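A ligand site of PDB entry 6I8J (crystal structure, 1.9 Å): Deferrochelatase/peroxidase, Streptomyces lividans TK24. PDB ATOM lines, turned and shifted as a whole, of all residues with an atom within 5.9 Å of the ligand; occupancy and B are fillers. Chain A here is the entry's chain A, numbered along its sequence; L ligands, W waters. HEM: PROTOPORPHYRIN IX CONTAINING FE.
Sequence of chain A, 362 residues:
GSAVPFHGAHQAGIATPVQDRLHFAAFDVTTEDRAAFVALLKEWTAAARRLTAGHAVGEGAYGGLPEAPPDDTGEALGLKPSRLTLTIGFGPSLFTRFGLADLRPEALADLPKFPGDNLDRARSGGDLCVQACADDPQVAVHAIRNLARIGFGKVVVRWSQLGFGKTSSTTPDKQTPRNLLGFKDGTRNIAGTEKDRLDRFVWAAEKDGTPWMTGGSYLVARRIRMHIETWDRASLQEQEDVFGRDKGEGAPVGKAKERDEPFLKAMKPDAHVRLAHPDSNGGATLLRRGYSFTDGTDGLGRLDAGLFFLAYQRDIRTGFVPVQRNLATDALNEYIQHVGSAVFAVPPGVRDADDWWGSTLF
An iron atom (FE) of the ligand is bound by a ring nitrogen (NE2) of His 272 (2.2 Å). O1A of the ligand is in hydrogen-bond range of N of Gly 186, 2.7 Å away. NE of Arg 188 is in salt-bridge range of O1D of the ligand, 2.8 Å away. NH1 of Arg 288 lies within salt-bridge range of O1A of the ligand (2.9 Å). The backbone NH of Arg 188 lies within hydrogen-bond range of an oxygen (O2A) of the ligand, at 2.9 Å. N of Thr 187 is in hydrogen-bond range of O1A of the ligand (3.3 Å).
O of Arg 188 sits at hydrogen-bond distance from NH2 of Arg 288, 3.0 Å away. ND2 of Asn 179 lies within hydrogen-bond range of OD2 of Asp 185 (2.6 Å). N of Val 273 sits at hydrogen-bond distance from O of Phe 243 (3.1 Å). A ring nitrogen (NE2) of His 277 sits at hydrogen-bond distance from the guanidinium group of Arg 188 (3.4 Å). N of Arg 288 sits at hydrogen-bond distance from OD1 of Asn 189 (2.8 Å). The side-chain amide oxygen (OD1) of Asn 179 lies within hydrogen-bond range of the backbone NH (N) of Phe 183. OD1 of Asn 179 sits at hydrogen-bond distance from N of Leu 181 (3.0 Å). The guanidinium group (NH1) of Arg 288 is in salt-bridge range of the side-chain carboxylate (OD1) of Asp 185 (3.1 Å).
Merely in contact with the ligand: Pro 278 (3.1 Å), Asp 185 (3.3 Å), Lys 184 (3.3 Å), His 277 (3.4 Å), Phe 320 (3.4 Å), Gln 324 (3.4 Å), Asn 179 (3.5 Å), Phe 243 (3.5 Å), Met 226 (3.5 Å), Ala 276 (3.5 Å), Phe 309 (3.5 Å), Leu 332 (3.7 Å), Val 273 (3.7 Å), Leu 181 (3.8 Å), Ile 336 (3.8 Å), Leu 327 (3.8 Å), Phe 183 (3.8 Å), Val 323 (3.9 Å) and Arg 245 (3.9 Å). Hydrophobic or aromatic side chains that line the ligand: Leu 181, Phe 183, Met 226, Phe 243, His 272, Val 273, Ala 276, His 277, Pro 278, Phe 309, Phe 320, Val 323, Leu 327, Leu 332 and Ile 336. Within 4 Å of the ligand: Asn 179, Leu 181, Phe 183, Lys 184, Asp 185, Gly 186, Thr 187, Arg 188, Met 226, Phe 243, Arg 245, His 272, Val 273, Ala 276, His 277, Pro 278, Arg 288, Phe 309, Phe 320, Val 323, Gln 324, Leu 327, Leu 332 and Ile 336. The nearest printed residue that does not touch the ligand is Leu 307 (4.02 Å).
Water W4 bridges an oxygen (O2D) of the ligand and the backbone carbonyl oxygen of Arg 188. Water W1 bridges an oxygen (O2A) of the ligand (2.8 Å) and the guanidinium group of Arg 245 (2.8 Å). Water W2 lies within hydrogen-bond range of the side-chain amide oxygen (OE1) of Gln 324 (2.9 Å) and a ring nitrogen (NE2) of His 338 (3.0 Å).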
ATOM      1  N   ASN A 179      22.213 -24.699  -7.728  1.00  0.00           N
ATOM      2  CA  ASN A 179      20.789 -24.910  -7.465  1.00  0.00           C
ATOM      3  C   ASN A 179      20.041 -25.051  -8.788  1.00  0.00           C
ATOM      4  O   ASN A 179      20.613 -24.925  -9.874  1.00  0.00           O
ATOM      5  CB  ASN A 179      20.194 -23.781  -6.623  1.00  0.00           C
ATOM      6  CG  ASN A 179      20.463 -22.405  -7.214  1.00  0.00           C
ATOM      7  OD1 ASN A 179      20.319 -22.182  -8.423  1.00  0.00           O
ATOM      8  ND2 ASN A 179      20.874 -21.489  -6.364  1.00  0.00           N
ATOM      9  N   LEU A 181      18.161 -23.123 -10.314  1.00  0.00           N
ATOM     10  CA  LEU A 181      18.239 -21.968 -11.209  1.00  0.00           C
ATOM     11  C   LEU A 181      19.535 -21.940 -12.008  1.00  0.00           C
ATOM     12  O   LEU A 181      19.722 -21.026 -12.814  1.00  0.00           O
ATOM     13  CB  LEU A 181      18.088 -20.677 -10.407  1.00  0.00           C
ATOM     14  CG  LEU A 181      16.817 -20.608  -9.537  1.00  0.00           C
ATOM     15  CD1 LEU A 181      16.675 -19.238  -8.883  1.00  0.00           C
ATOM     16  CD2 LEU A 181      15.593 -20.909 -10.395  1.00  0.00           C
ATOM     17  N   PHE A 183      22.684 -21.580 -10.800  1.00  0.00           N
ATOM     18  CA  PHE A 183      23.743 -20.760 -10.231  1.00  0.00           C
ATOM     19  C   PHE A 183      24.454 -21.517  -9.106  1.00  0.00           C
ATOM     20  O   PHE A 183      23.824 -22.267  -8.364  1.00  0.00           O
ATOM     21  CB  PHE A 183      23.182 -19.433  -9.697  1.00  0.00           C
ATOM     22  CG  PHE A 183      22.970 -18.391 -10.773  1.00  0.00           C
ATOM     23  CD1 PHE A 183      21.881 -18.483 -11.661  1.00  0.00           C
ATOM     24  CD2 PHE A 183      23.836 -17.329 -10.904  1.00  0.00           C
ATOM     25  CE1 PHE A 183      21.684 -17.529 -12.661  1.00  0.00           C
ATOM     26  CE2 PHE A 183      23.641 -16.355 -11.900  1.00  0.00           C
ATOM     27  CZ  PHE A 183      22.569 -16.471 -12.780  1.00  0.00           C
ATOM     28  N   LYS A 184      25.776 -21.334  -9.016  1.00  0.00           N
ATOM     29  CA  LYS A 184      26.498 -21.864  -7.858  1.00  0.00           C
ATOM     30  C   LYS A 184      25.916 -21.268  -6.590  1.00  0.00           C
ATOM     31  O   LYS A 184      25.631 -20.070  -6.522  1.00  0.00           O
ATOM     32  CB  LYS A 184      27.999 -21.551  -7.941  1.00  0.00           C
ATOM     33  CG  LYS A 184      28.718 -22.150  -9.155  1.00  0.00           C
ATOM     34  CD  LYS A 184      30.136 -21.588  -9.272  1.00  0.00           C
ATOM     35  CE  LYS A 184      31.013 -22.474 -10.176  1.00  0.00           C
ATOM     36  NZ  LYS A 184      32.348 -21.856 -10.444  1.00  0.00           N
ATOM     37  N   ASP A 185      25.730 -22.109  -5.577  1.00  0.00           N
ATOM     38  CA  ASP A 185      25.079 -21.706  -4.332  1.00  0.00           C
ATOM     39  C   ASP A 185      25.947 -22.198  -3.173  1.00  0.00           C
ATOM     40  O   ASP A 185      26.142 -23.410  -3.017  1.00  0.00           O
ATOM     41  CB  ASP A 185      23.660 -22.311  -4.253  1.00  0.00           C
ATOM     42  CG  ASP A 185      22.659 -21.443  -3.467  1.00  0.00           C
ATOM     43  OD1 ASP A 185      23.045 -20.835  -2.440  1.00  0.00           O
ATOM     44  OD2 ASP A 185      21.478 -21.382  -3.886  1.00  0.00           O
ATOM     45  N   GLY A 186      26.473 -21.273  -2.372  1.00  0.00           N
ATOM     46  CA  GLY A 186      27.327 -21.634  -1.252  1.00  0.00           C
ATOM     47  C   GLY A 186      28.715 -20.997  -1.267  1.00  0.00           C
ATOM     48  O   GLY A 186      29.513 -21.271  -0.361  1.00  0.00           O
ATOM     49  N   THR A 187      29.031 -20.126  -2.231  1.00  0.00           N
ATOM     50  CA  THR A 187      30.386 -19.581  -2.338  1.00  0.00           C
ATOM     51  C   THR A 187      30.804 -18.870  -1.065  1.00  0.00           C
ATOM     52  O   THR A 187      31.807 -19.222  -0.429  1.00  0.00           O
ATOM     53  CB  THR A 187      30.476 -18.635  -3.535  1.00  0.00           C
ATOM     54  OG1 THR A 187      30.111 -19.359  -4.713  1.00  0.00           O
ATOM     55  CG2 THR A 187      31.888 -18.075  -3.694  1.00  0.00           C
ATOM     56  N   ARG A 188      30.017 -17.869  -0.642  1.00  0.00           N
ATOM     57  CA  ARG A 188      30.316 -17.093   0.560  1.00  0.00           C
ATOM     58  C   ARG A 188      29.401 -17.575   1.690  1.00  0.00           C
ATOM     59  O   ARG A 188      28.399 -16.951   2.043  1.00  0.00           O
ATOM     60  CB  ARG A 188      30.198 -15.592   0.301  1.00  0.00           C
ATOM     61  CG  ARG A 188      31.369 -15.045  -0.538  1.00  0.00           C
ATOM     62  CD  ARG A 188      31.390 -13.506  -0.582  1.00  0.00           C
ATOM     63  NE  ARG A 188      30.745 -12.982   0.615  1.00  0.00           N
ATOM     64  CZ  ARG A 188      31.377 -12.659   1.735  1.00  0.00           C
ATOM     65  NH1 ARG A 188      30.686 -12.213   2.771  1.00  0.00           N
ATOM     66  NH2 ARG A 188      32.709 -12.773   1.823  1.00  0.00           N
ATOM     67  N   ASN A 189      29.775 -18.707   2.255  1.00  0.00           N
ATOM     68  CA  ASN A 189      29.130 -19.298   3.402  1.00  0.00           C
ATOM     69  C   ASN A 189      30.156 -19.347   4.524  1.00  0.00           C
ATOM     70  O   ASN A 189      31.284 -18.888   4.380  1.00  0.00           O
ATOM     71  CB  ASN A 189      28.593 -20.681   3.027  1.00  0.00           C
ATOM     72  CG  ASN A 189      27.511 -21.173   3.966  1.00  0.00           C
ATOM     73  OD1 ASN A 189      26.698 -20.393   4.427  1.00  0.00           O
ATOM     74  ND2 ASN A 189      27.487 -22.478   4.226  1.00  0.00           N
ATOM     75  N   ILE A 224      10.851 -23.339  -0.280  1.00  0.00           N
ATOM     76  CA  ILE A 224      10.768 -22.221  -1.228  1.00  0.00           C
ATOM     77  C   ILE A 224      10.528 -22.771  -2.628  1.00  0.00           C
ATOM     78  O   ILE A 224      11.420 -23.379  -3.224  1.00  0.00           O
ATOM     79  CB  ILE A 224      12.017 -21.335  -1.201  1.00  0.00           C
ATOM     80  CG1 ILE A 224      12.271 -20.898   0.251  1.00  0.00           C
ATOM     81  CG2 ILE A 224      11.840 -20.140  -2.134  1.00  0.00           C
ATOM     82  CD1 ILE A 224      13.592 -20.146   0.465  1.00  0.00           C
ATOM     83  N   ARG A 225       9.336 -22.522  -3.168  1.00  0.00           N
ATOM     84  CA  ARG A 225       9.019 -22.909  -4.525  1.00  0.00           C
ATOM     85  C   ARG A 225       9.698 -21.954  -5.510  1.00  0.00           C
ATOM     86  O   ARG A 225       9.794 -20.751  -5.272  1.00  0.00           O
ATOM     87  CB  ARG A 225       7.505 -22.888  -4.739  1.00  0.00           C
ATOM     88  CG  ARG A 225       7.042 -23.340  -6.122  1.00  0.00           C
ATOM     89  CD  ARG A 225       6.294 -24.659  -6.037  1.00  0.00           C
ATOM     90  NE  ARG A 225       5.029 -24.545  -5.301  1.00  0.00           N
ATOM     91  CZ  ARG A 225       4.566 -25.461  -4.462  1.00  0.00           C
ATOM     92  NH1 ARG A 225       5.269 -26.579  -4.229  1.00  0.00           N
ATOM     93  NH2 ARG A 225       3.398 -25.271  -3.846  1.00  0.00           N
ATOM     94  N   MET A 226      10.162 -22.507  -6.628  1.00  0.00           N
ATOM     95  CA  MET A 226      10.761 -21.721  -7.703  1.00  0.00           C
ATOM     96  C   MET A 226       9.848 -21.724  -8.926  1.00  0.00           C
ATOM     97  O   MET A 226       9.369 -22.785  -9.359  1.00  0.00           O
ATOM     98  CB  MET A 226      12.129 -22.247  -8.095  1.00  0.00           C
ATOM     99  CG  MET A 226      13.185 -22.138  -7.013  1.00  0.00           C
ATOM    100  SD  MET A 226      14.554 -23.262  -7.432  1.00  0.00           S
ATOM    101  CE  MET A 226      15.843 -22.531  -6.449  1.00  0.00           C
ATOM    102  N   PHE A 243      21.136 -11.842  -9.493  1.00  0.00           N
ATOM    103  CA  PHE A 243      21.992 -12.297  -8.410  1.00  0.00           C
ATOM    104  C   PHE A 243      23.160 -11.354  -8.166  1.00  0.00           C
ATOM    105  O   PHE A 243      23.528 -11.115  -7.015  1.00  0.00           O
ATOM    106  CB  PHE A 243      22.505 -13.716  -8.711  1.00  0.00           C
ATOM    107  CG  PHE A 243      21.487 -14.773  -8.430  1.00  0.00           C
ATOM    108  CD1 PHE A 243      21.059 -15.003  -7.135  1.00  0.00           C
ATOM    109  CD2 PHE A 243      20.937 -15.508  -9.465  1.00  0.00           C
ATOM    110  CE1 PHE A 243      20.092 -15.961  -6.862  1.00  0.00           C
ATOM    111  CE2 PHE A 243      19.963 -16.452  -9.211  1.00  0.00           C
ATOM    112  CZ  PHE A 243      19.552 -16.697  -7.896  1.00  0.00           C
ATOM    113  N   ARG A 245      26.052 -12.107  -9.789  1.00  0.00           N
ATOM    114  CA  ARG A 245      27.179 -12.927 -10.187  1.00  0.00           C
ATOM    115  C   ARG A 245      26.838 -13.462 -11.563  1.00  0.00           C
ATOM    116  O   ARG A 245      25.666 -13.565 -11.930  1.00  0.00           O
ATOM    117  CB  ARG A 245      27.436 -14.079  -9.197  1.00  0.00           C
ATOM    118  CG  ARG A 245      27.854 -13.650  -7.782  1.00  0.00           C
ATOM    119  CD  ARG A 245      28.083 -14.878  -6.912  1.00  0.00           C
ATOM    120  NE  ARG A 245      28.637 -14.565  -5.596  1.00  0.00           N
ATOM    121  CZ  ARG A 245      29.937 -14.652  -5.312  1.00  0.00           C
ATOM    122  NH1 ARG A 245      30.797 -15.032  -6.237  1.00  0.00           N
ATOM    123  NH2 ARG A 245      30.375 -14.363  -4.084  1.00  0.00           N
ATOM    124  N   PRO A 262      33.092  -9.862  -3.756  1.00  0.00           N
ATOM    125  CA  PRO A 262      32.135  -9.020  -4.461  1.00  0.00           C
ATOM    126  C   PRO A 262      32.418  -7.543  -4.195  1.00  0.00           C
ATOM    127  O   PRO A 262      32.806  -7.153  -3.096  1.00  0.00           O
ATOM    128  CB  PRO A 262      30.785  -9.451  -3.884  1.00  0.00           C
ATOM    129  CG  PRO A 262      31.104 -10.216  -2.645  1.00  0.00           C
ATOM    130  CD  PRO A 262      32.448 -10.818  -2.839  1.00  0.00           C
ATOM    131  N   HIS A 272      20.345  -9.948  -5.395  1.00  0.00           N
ATOM    132  CA  HIS A 272      20.235 -10.823  -4.238  1.00  0.00           C
ATOM    133  C   HIS A 272      21.493 -10.790  -3.385  1.00  0.00           C
ATOM    134  O   HIS A 272      21.416 -10.617  -2.166  1.00  0.00           O
ATOM    135  CB  HIS A 272      19.943 -12.252  -4.700  1.00  0.00           C
ATOM    136  CG  HIS A 272      19.776 -13.224  -3.597  1.00  0.00           C
ATOM    137  ND1 HIS A 272      18.598 -13.358  -2.888  1.00  0.00           N
ATOM    138  CD2 HIS A 272      20.630 -14.142  -3.089  1.00  0.00           C
ATOM    139  CE1 HIS A 272      18.732 -14.308  -1.986  1.00  0.00           C
ATOM    140  NE2 HIS A 272      19.959 -14.797  -2.079  1.00  0.00           N
ATOM    141  N   VAL A 273      22.667 -10.927  -4.011  1.00  0.00           N
ATOM    142  CA  VAL A 273      23.918 -10.928  -3.247  1.00  0.00           C
ATOM    143  C   VAL A 273      24.113  -9.586  -2.554  1.00  0.00           C
ATOM    144  O   VAL A 273      24.533  -9.518  -1.388  1.00  0.00           O
ATOM    145  CB  VAL A 273      25.113 -11.278  -4.164  1.00  0.00           C
ATOM    146  CG1 VAL A 273      26.442 -10.958  -3.457  1.00  0.00           C
ATOM    147  CG2 VAL A 273      25.054 -12.740  -4.559  1.00  0.00           C
ATOM    148  N   ALA A 276      21.741  -9.585   0.575  1.00  0.00           N
ATOM    149  CA  ALA A 276      22.043 -10.599   1.573  1.00  0.00           C
ATOM    150  C   ALA A 276      23.429 -10.481   2.189  1.00  0.00           C
ATOM    151  O   ALA A 276      23.661 -11.016   3.278  1.00  0.00           O
ATOM    152  CB  ALA A 276      21.895 -12.003   0.966  1.00  0.00           C
ATOM    153  N   HIS A 277      24.340  -9.763   1.540  1.00  0.00           N
ATOM    154  CA  HIS A 277      25.723  -9.687   2.004  1.00  0.00           C
ATOM    155  C   HIS A 277      25.762  -9.189   3.447  1.00  0.00           C
ATOM    156  O   HIS A 277      24.954  -8.333   3.831  1.00  0.00           O
ATOM    157  CB  HIS A 277      26.525  -8.766   1.086  1.00  0.00           C
ATOM    158  CG  HIS A 277      28.010  -8.916   1.243  1.00  0.00           C
ATOM    159  ND1 HIS A 277      28.714  -8.339   2.285  1.00  0.00           N
ATOM    160  CD2 HIS A 277      28.933  -9.546   0.473  1.00  0.00           C
ATOM    161  CE1 HIS A 277      29.994  -8.633   2.161  1.00  0.00           C
ATOM    162  NE2 HIS A 277      30.154  -9.369   1.073  1.00  0.00           N
ATOM    163  N   PRO A 278      26.661  -9.715   4.286  1.00  0.00           N
ATOM    164  CA  PRO A 278      26.736  -9.209   5.672  1.00  0.00           C
ATOM    165  C   PRO A 278      26.944  -7.704   5.772  1.00  0.00           C
ATOM    166  O   PRO A 278      26.395  -7.061   6.673  1.00  0.00           O
ATOM    167  CB  PRO A 278      27.921  -9.987   6.257  1.00  0.00           C
ATOM    168  CG  PRO A 278      27.905 -11.270   5.542  1.00  0.00           C
ATOM    169  CD  PRO A 278      27.444 -10.949   4.126  1.00  0.00           C
ATOM    170  N   LEU A 286      25.082 -15.986   8.218  1.00  0.00           N
ATOM    171  CA  LEU A 286      24.330 -17.220   8.339  1.00  0.00           C
ATOM    172  C   LEU A 286      25.173 -18.401   7.869  1.00  0.00           C
ATOM    173  O   LEU A 286      26.043 -18.233   7.014  1.00  0.00           O
ATOM    174  CB  LEU A 286      23.069 -17.192   7.487  1.00  0.00           C
ATOM    175  CG  LEU A 286      22.094 -16.057   7.773  1.00  0.00           C
ATOM    176  CD1 LEU A 286      20.932 -16.136   6.798  1.00  0.00           C
ATOM    177  CD2 LEU A 286      21.593 -16.198   9.230  1.00  0.00           C
ATOM    178  N   ARG A 288      24.388 -21.409   5.682  1.00  0.00           N
ATOM    179  CA  ARG A 288      23.378 -21.991   4.805  1.00  0.00           C
ATOM    180  C   ARG A 288      23.688 -23.474   4.564  1.00  0.00           C
ATOM    181  O   ARG A 288      24.852 -23.859   4.383  1.00  0.00           O
ATOM    182  CB  ARG A 288      23.319 -21.214   3.491  1.00  0.00           C
ATOM    183  CG  ARG A 288      22.557 -19.903   3.615  1.00  0.00           C
ATOM    184  CD  ARG A 288      22.714 -19.019   2.392  1.00  0.00           C
ATOM    185  NE  ARG A 288      24.102 -18.637   2.157  1.00  0.00           N
ATOM    186  CZ  ARG A 288      24.706 -18.677   0.963  1.00  0.00           C
ATOM    187  NH1 ARG A 288      24.035 -19.065  -0.123  1.00  0.00           N
ATOM    188  NH2 ARG A 288      25.983 -18.308   0.847  1.00  0.00           N
ATOM    189  N   LEU A 307      13.636 -25.160  -3.487  1.00  0.00           N
ATOM    190  CA  LEU A 307      14.805 -25.210  -2.637  1.00  0.00           C
ATOM    191  C   LEU A 307      14.343 -25.271  -1.192  1.00  0.00           C
ATOM    192  O   LEU A 307      13.515 -24.464  -0.758  1.00  0.00           O
ATOM    193  CB  LEU A 307      15.713 -24.009  -2.871  1.00  0.00           C
ATOM    194  CG  LEU A 307      17.073 -24.087  -2.182  1.00  0.00           C
ATOM    195  CD1 LEU A 307      18.181 -23.655  -3.139  1.00  0.00           C
ATOM    196  CD2 LEU A 307      17.085 -23.215  -0.919  1.00  0.00           C
ATOM    197  N   PHE A 309      15.361 -24.489   2.163  1.00  0.00           N
ATOM    198  CA  PHE A 309      16.368 -23.599   2.709  1.00  0.00           C
ATOM    199  C   PHE A 309      16.529 -23.836   4.203  1.00  0.00           C
ATOM    200  O   PHE A 309      15.552 -23.844   4.964  1.00  0.00           O
ATOM    201  CB  PHE A 309      15.986 -22.142   2.427  1.00  0.00           C
ATOM    202  CG  PHE A 309      16.966 -21.134   2.961  1.00  0.00           C
ATOM    203  CD1 PHE A 309      18.033 -20.679   2.167  1.00  0.00           C
ATOM    204  CD2 PHE A 309      16.811 -20.596   4.228  1.00  0.00           C
ATOM    205  CE1 PHE A 309      18.938 -19.739   2.661  1.00  0.00           C
ATOM    206  CE2 PHE A 309      17.707 -19.647   4.733  1.00  0.00           C
ATOM    207  CZ  PHE A 309      18.771 -19.213   3.945  1.00  0.00           C
ATOM    208  N   PHE A 320      18.673 -14.832  10.595  1.00  0.00           N
ATOM    209  CA  PHE A 320      17.765 -14.922   9.449  1.00  0.00           C
ATOM    210  C   PHE A 320      16.847 -13.721   9.364  1.00  0.00           C
ATOM    211  O   PHE A 320      16.571 -13.213   8.276  1.00  0.00           O
ATOM    212  CB  PHE A 320      16.968 -16.226   9.532  1.00  0.00           C
ATOM    213  CG  PHE A 320      15.917 -16.363   8.486  1.00  0.00           C
ATOM    214  CD1 PHE A 320      14.622 -15.927   8.726  1.00  0.00           C
ATOM    215  CD2 PHE A 320      16.191 -16.965   7.280  1.00  0.00           C
ATOM    216  CE1 PHE A 320      13.634 -16.066   7.768  1.00  0.00           C
ATOM    217  CE2 PHE A 320      15.213 -17.120   6.299  1.00  0.00           C
ATOM    218  CZ  PHE A 320      13.930 -16.666   6.544  1.00  0.00           C
ATOM    219  N   VAL A 323      18.321 -10.415   7.638  1.00  0.00           N
ATOM    220  CA  VAL A 323      18.636 -10.668   6.244  1.00  0.00           C
ATOM    221  C   VAL A 323      17.359 -10.858   5.422  1.00  0.00           C
ATOM    222  O   VAL A 323      17.190 -10.281   4.347  1.00  0.00           O
ATOM    223  CB  VAL A 323      19.589 -11.882   6.115  1.00  0.00           C
ATOM    224  CG1 VAL A 323      19.942 -12.121   4.636  1.00  0.00           C
ATOM    225  CG2 VAL A 323      20.881 -11.650   6.926  1.00  0.00           C
ATOM    226  N   GLN A 324      16.420 -11.659   5.930  1.00  0.00           N
ATOM    227  CA  GLN A 324      15.181 -11.825   5.178  1.00  0.00           C
ATOM    228  C   GLN A 324      14.373 -10.525   5.111  1.00  0.00           C
ATOM    229  O   GLN A 324      13.669 -10.276   4.129  1.00  0.00           O
ATOM    230  CB  GLN A 324      14.323 -12.955   5.767  1.00  0.00           C
ATOM    231  CG  GLN A 324      12.979 -13.138   5.042  1.00  0.00           C
ATOM    232  CD  GLN A 324      13.096 -13.750   3.645  1.00  0.00           C
ATOM    233  OE1 GLN A 324      14.046 -14.449   3.334  1.00  0.00           O
ATOM    234  NE2 GLN A 324      12.085 -13.532   2.810  1.00  0.00           N
ATOM    235  N   LEU A 327      15.585  -8.616   2.309  1.00  0.00           N
ATOM    236  CA  LEU A 327      15.265  -9.188   1.010  1.00  0.00           C
ATOM    237  C   LEU A 327      13.873  -8.786   0.509  1.00  0.00           C
ATOM    238  O   LEU A 327      13.453  -9.263  -0.547  1.00  0.00           O
ATOM    239  CB  LEU A 327      15.385 -10.713   1.071  1.00  0.00           C
ATOM    240  CG  LEU A 327      16.801 -11.231   1.369  1.00  0.00           C
ATOM    241  CD1 LEU A 327      16.837 -12.765   1.461  1.00  0.00           C
ATOM    242  CD2 LEU A 327      17.770 -10.756   0.304  1.00  0.00           C
ATOM    243  N   LEU A 332      15.144 -11.354  -6.758  1.00  0.00           N
ATOM    244  CA  LEU A 332      14.822 -12.773  -6.833  1.00  0.00           C
ATOM    245  C   LEU A 332      13.361 -13.063  -6.456  1.00  0.00           C
ATOM    246  O   LEU A 332      12.839 -14.111  -6.830  1.00  0.00           O
ATOM    247  CB  LEU A 332      15.770 -13.551  -5.923  1.00  0.00           C
ATOM    248  CG  LEU A 332      15.599 -15.069  -5.869  1.00  0.00           C
ATOM    249  CD1 LEU A 332      15.841 -15.718  -7.240  1.00  0.00           C
ATOM    250  CD2 LEU A 332      16.524 -15.652  -4.793  1.00  0.00           C
ATOM    251  N   ILE A 336      10.440 -16.748  -6.839  1.00  0.00           N
ATOM    252  CA  ILE A 336      10.337 -17.712  -5.758  1.00  0.00           C
ATOM    253  C   ILE A 336       9.114 -17.388  -4.909  1.00  0.00           C
ATOM    254  O   ILE A 336       8.536 -16.301  -4.981  1.00  0.00           O
ATOM    255  CB  ILE A 336      11.597 -17.718  -4.861  1.00  0.00           C
ATOM    256  CG1 ILE A 336      11.765 -16.351  -4.177  1.00  0.00           C
ATOM    257  CG2 ILE A 336      12.834 -18.079  -5.685  1.00  0.00           C
ATOM    258  CD1 ILE A 336      12.862 -16.337  -3.098  1.00  0.00           C
ATOM    259  N   HIS A 338       7.910 -18.433  -0.693  1.00  0.00           N
ATOM    260  CA  HIS A 338       8.077 -19.212   0.530  1.00  0.00           C
ATOM    261  C   HIS A 338       6.754 -19.872   0.853  1.00  0.00           C
ATOM    262  O   HIS A 338       5.724 -19.186   1.000  1.00  0.00           O
ATOM    263  CB  HIS A 338       8.534 -18.317   1.676  1.00  0.00           C
ATOM    264  CG  HIS A 338       9.931 -17.797   1.518  1.00  0.00           C
ATOM    265  ND1 HIS A 338      10.931 -18.052   2.447  1.00  0.00           N
ATOM    266  CD2 HIS A 338      10.489 -17.019   0.560  1.00  0.00           C
ATOM    267  CE1 HIS A 338      12.041 -17.461   2.050  1.00  0.00           C
ATOM    268  NE2 HIS A 338      11.803 -16.815   0.919  1.00  0.00           N
HETATM  269  CHA HEM L   1      24.086 -16.034  -1.679  1.00  0.00           C
HETATM  270  CHB HEM L   1      20.695 -18.256  -4.322  1.00  0.00           C
HETATM  271  CHC HEM L   1      17.459 -17.742  -0.805  1.00  0.00           C
HETATM  272  CHD HEM L   1      20.913 -15.639   1.894  1.00  0.00           C
HETATM  273  C1A HEM L   1      23.437 -16.651  -2.702  1.00  0.00           C
HETATM  274  C2A HEM L   1      23.990 -16.878  -4.017  1.00  0.00           C
HETATM  275  C3A HEM L   1      23.049 -17.463  -4.746  1.00  0.00           C
HETATM  276  C4A HEM L   1      21.875 -17.661  -3.916  1.00  0.00           C
HETATM  277  CMA HEM L   1      23.167 -17.919  -6.216  1.00  0.00           C
HETATM  278  CAA HEM L   1      25.409 -16.459  -4.457  1.00  0.00           C
HETATM  279  CBA HEM L   1      26.476 -17.520  -4.159  1.00  0.00           C
HETATM  280  CGA HEM L   1      26.740 -17.753  -2.685  1.00  0.00           C
HETATM  281  O1A HEM L   1      26.106 -18.657  -2.094  1.00  0.00           O
HETATM  282  O2A HEM L   1      27.626 -17.041  -2.112  1.00  0.00           O
HETATM  283  C1B HEM L   1      19.533 -18.330  -3.611  1.00  0.00           C
HETATM  284  C2B HEM L   1      18.295 -18.943  -4.057  1.00  0.00           C
HETATM  285  C3B HEM L   1      17.389 -18.773  -3.083  1.00  0.00           C
HETATM  286  C4B HEM L   1      18.031 -18.076  -1.995  1.00  0.00           C
HETATM  287  CMB HEM L   1      18.111 -19.614  -5.433  1.00  0.00           C
HETATM  288  CAB HEM L   1      15.914 -19.254  -3.038  1.00  0.00           C
HETATM  289  CBB HEM L   1      15.460 -20.136  -3.936  1.00  0.00           C
HETATM  290  C1C HEM L   1      18.119 -17.117   0.220  1.00  0.00           C
HETATM  291  C2C HEM L   1      17.529 -16.709   1.463  1.00  0.00           C
HETATM  292  C3C HEM L   1      18.489 -16.128   2.203  1.00  0.00           C
HETATM  293  C4C HEM L   1      19.706 -16.142   1.450  1.00  0.00           C
HETATM  294  CMC HEM L   1      16.037 -16.947   1.795  1.00  0.00           C
HETATM  295  CAC HEM L   1      18.402 -15.510   3.614  1.00  0.00           C
HETATM  296  CBC HEM L   1      17.213 -15.354   4.201  1.00  0.00           C
HETATM  297  C1D HEM L   1      22.075 -15.583   1.169  1.00  0.00           C
HETATM  298  C2D HEM L   1      23.352 -15.137   1.670  1.00  0.00           C
HETATM  299  C3D HEM L   1      24.247 -15.221   0.680  1.00  0.00           C
HETATM  300  C4D HEM L   1      23.546 -15.758  -0.466  1.00  0.00           C
HETATM  301  CMD HEM L   1      23.620 -14.592   3.082  1.00  0.00           C
HETATM  302  CAD HEM L   1      25.729 -14.835   0.812  1.00  0.00           C
HETATM  303  CBD HEM L   1      25.985 -13.397   0.333  1.00  0.00           C
HETATM  304  CGD HEM L   1      27.409 -12.981   0.598  1.00  0.00           C
HETATM  305  O1D HEM L   1      28.167 -12.729  -0.375  1.00  0.00           O
HETATM  306  O2D HEM L   1      27.795 -12.935   1.787  1.00  0.00           O
HETATM  307  NA  HEM L   1      22.134 -17.134  -2.671  1.00  0.00           N
HETATM  308  NB  HEM L   1      19.336 -17.809  -2.340  1.00  0.00           N
HETATM  309  NC  HEM L   1      19.454 -16.760   0.251  1.00  0.00           N
HETATM  310  ND  HEM L   1      22.236 -15.982  -0.134  1.00  0.00           N
HETATM  311 FE   HEM L   1      20.714 -16.769  -1.303  1.00  0.00          FE
HETATM  312  O   HOH W   1      27.877 -14.296  -2.741  1.00  0.00           O
HETATM  313  O   HOH W   2      13.812 -14.682   0.481  1.00  0.00           O
HETATM  314  O   HOH W   3      24.302 -12.620   5.611  1.00  0.00           O
HETATM  315  O   HOH W   4      28.098 -14.596   3.709  1.00  0.00           O
HETATM  316  O   HOH W   5      25.732 -14.907   5.578  1.00  0.00           O
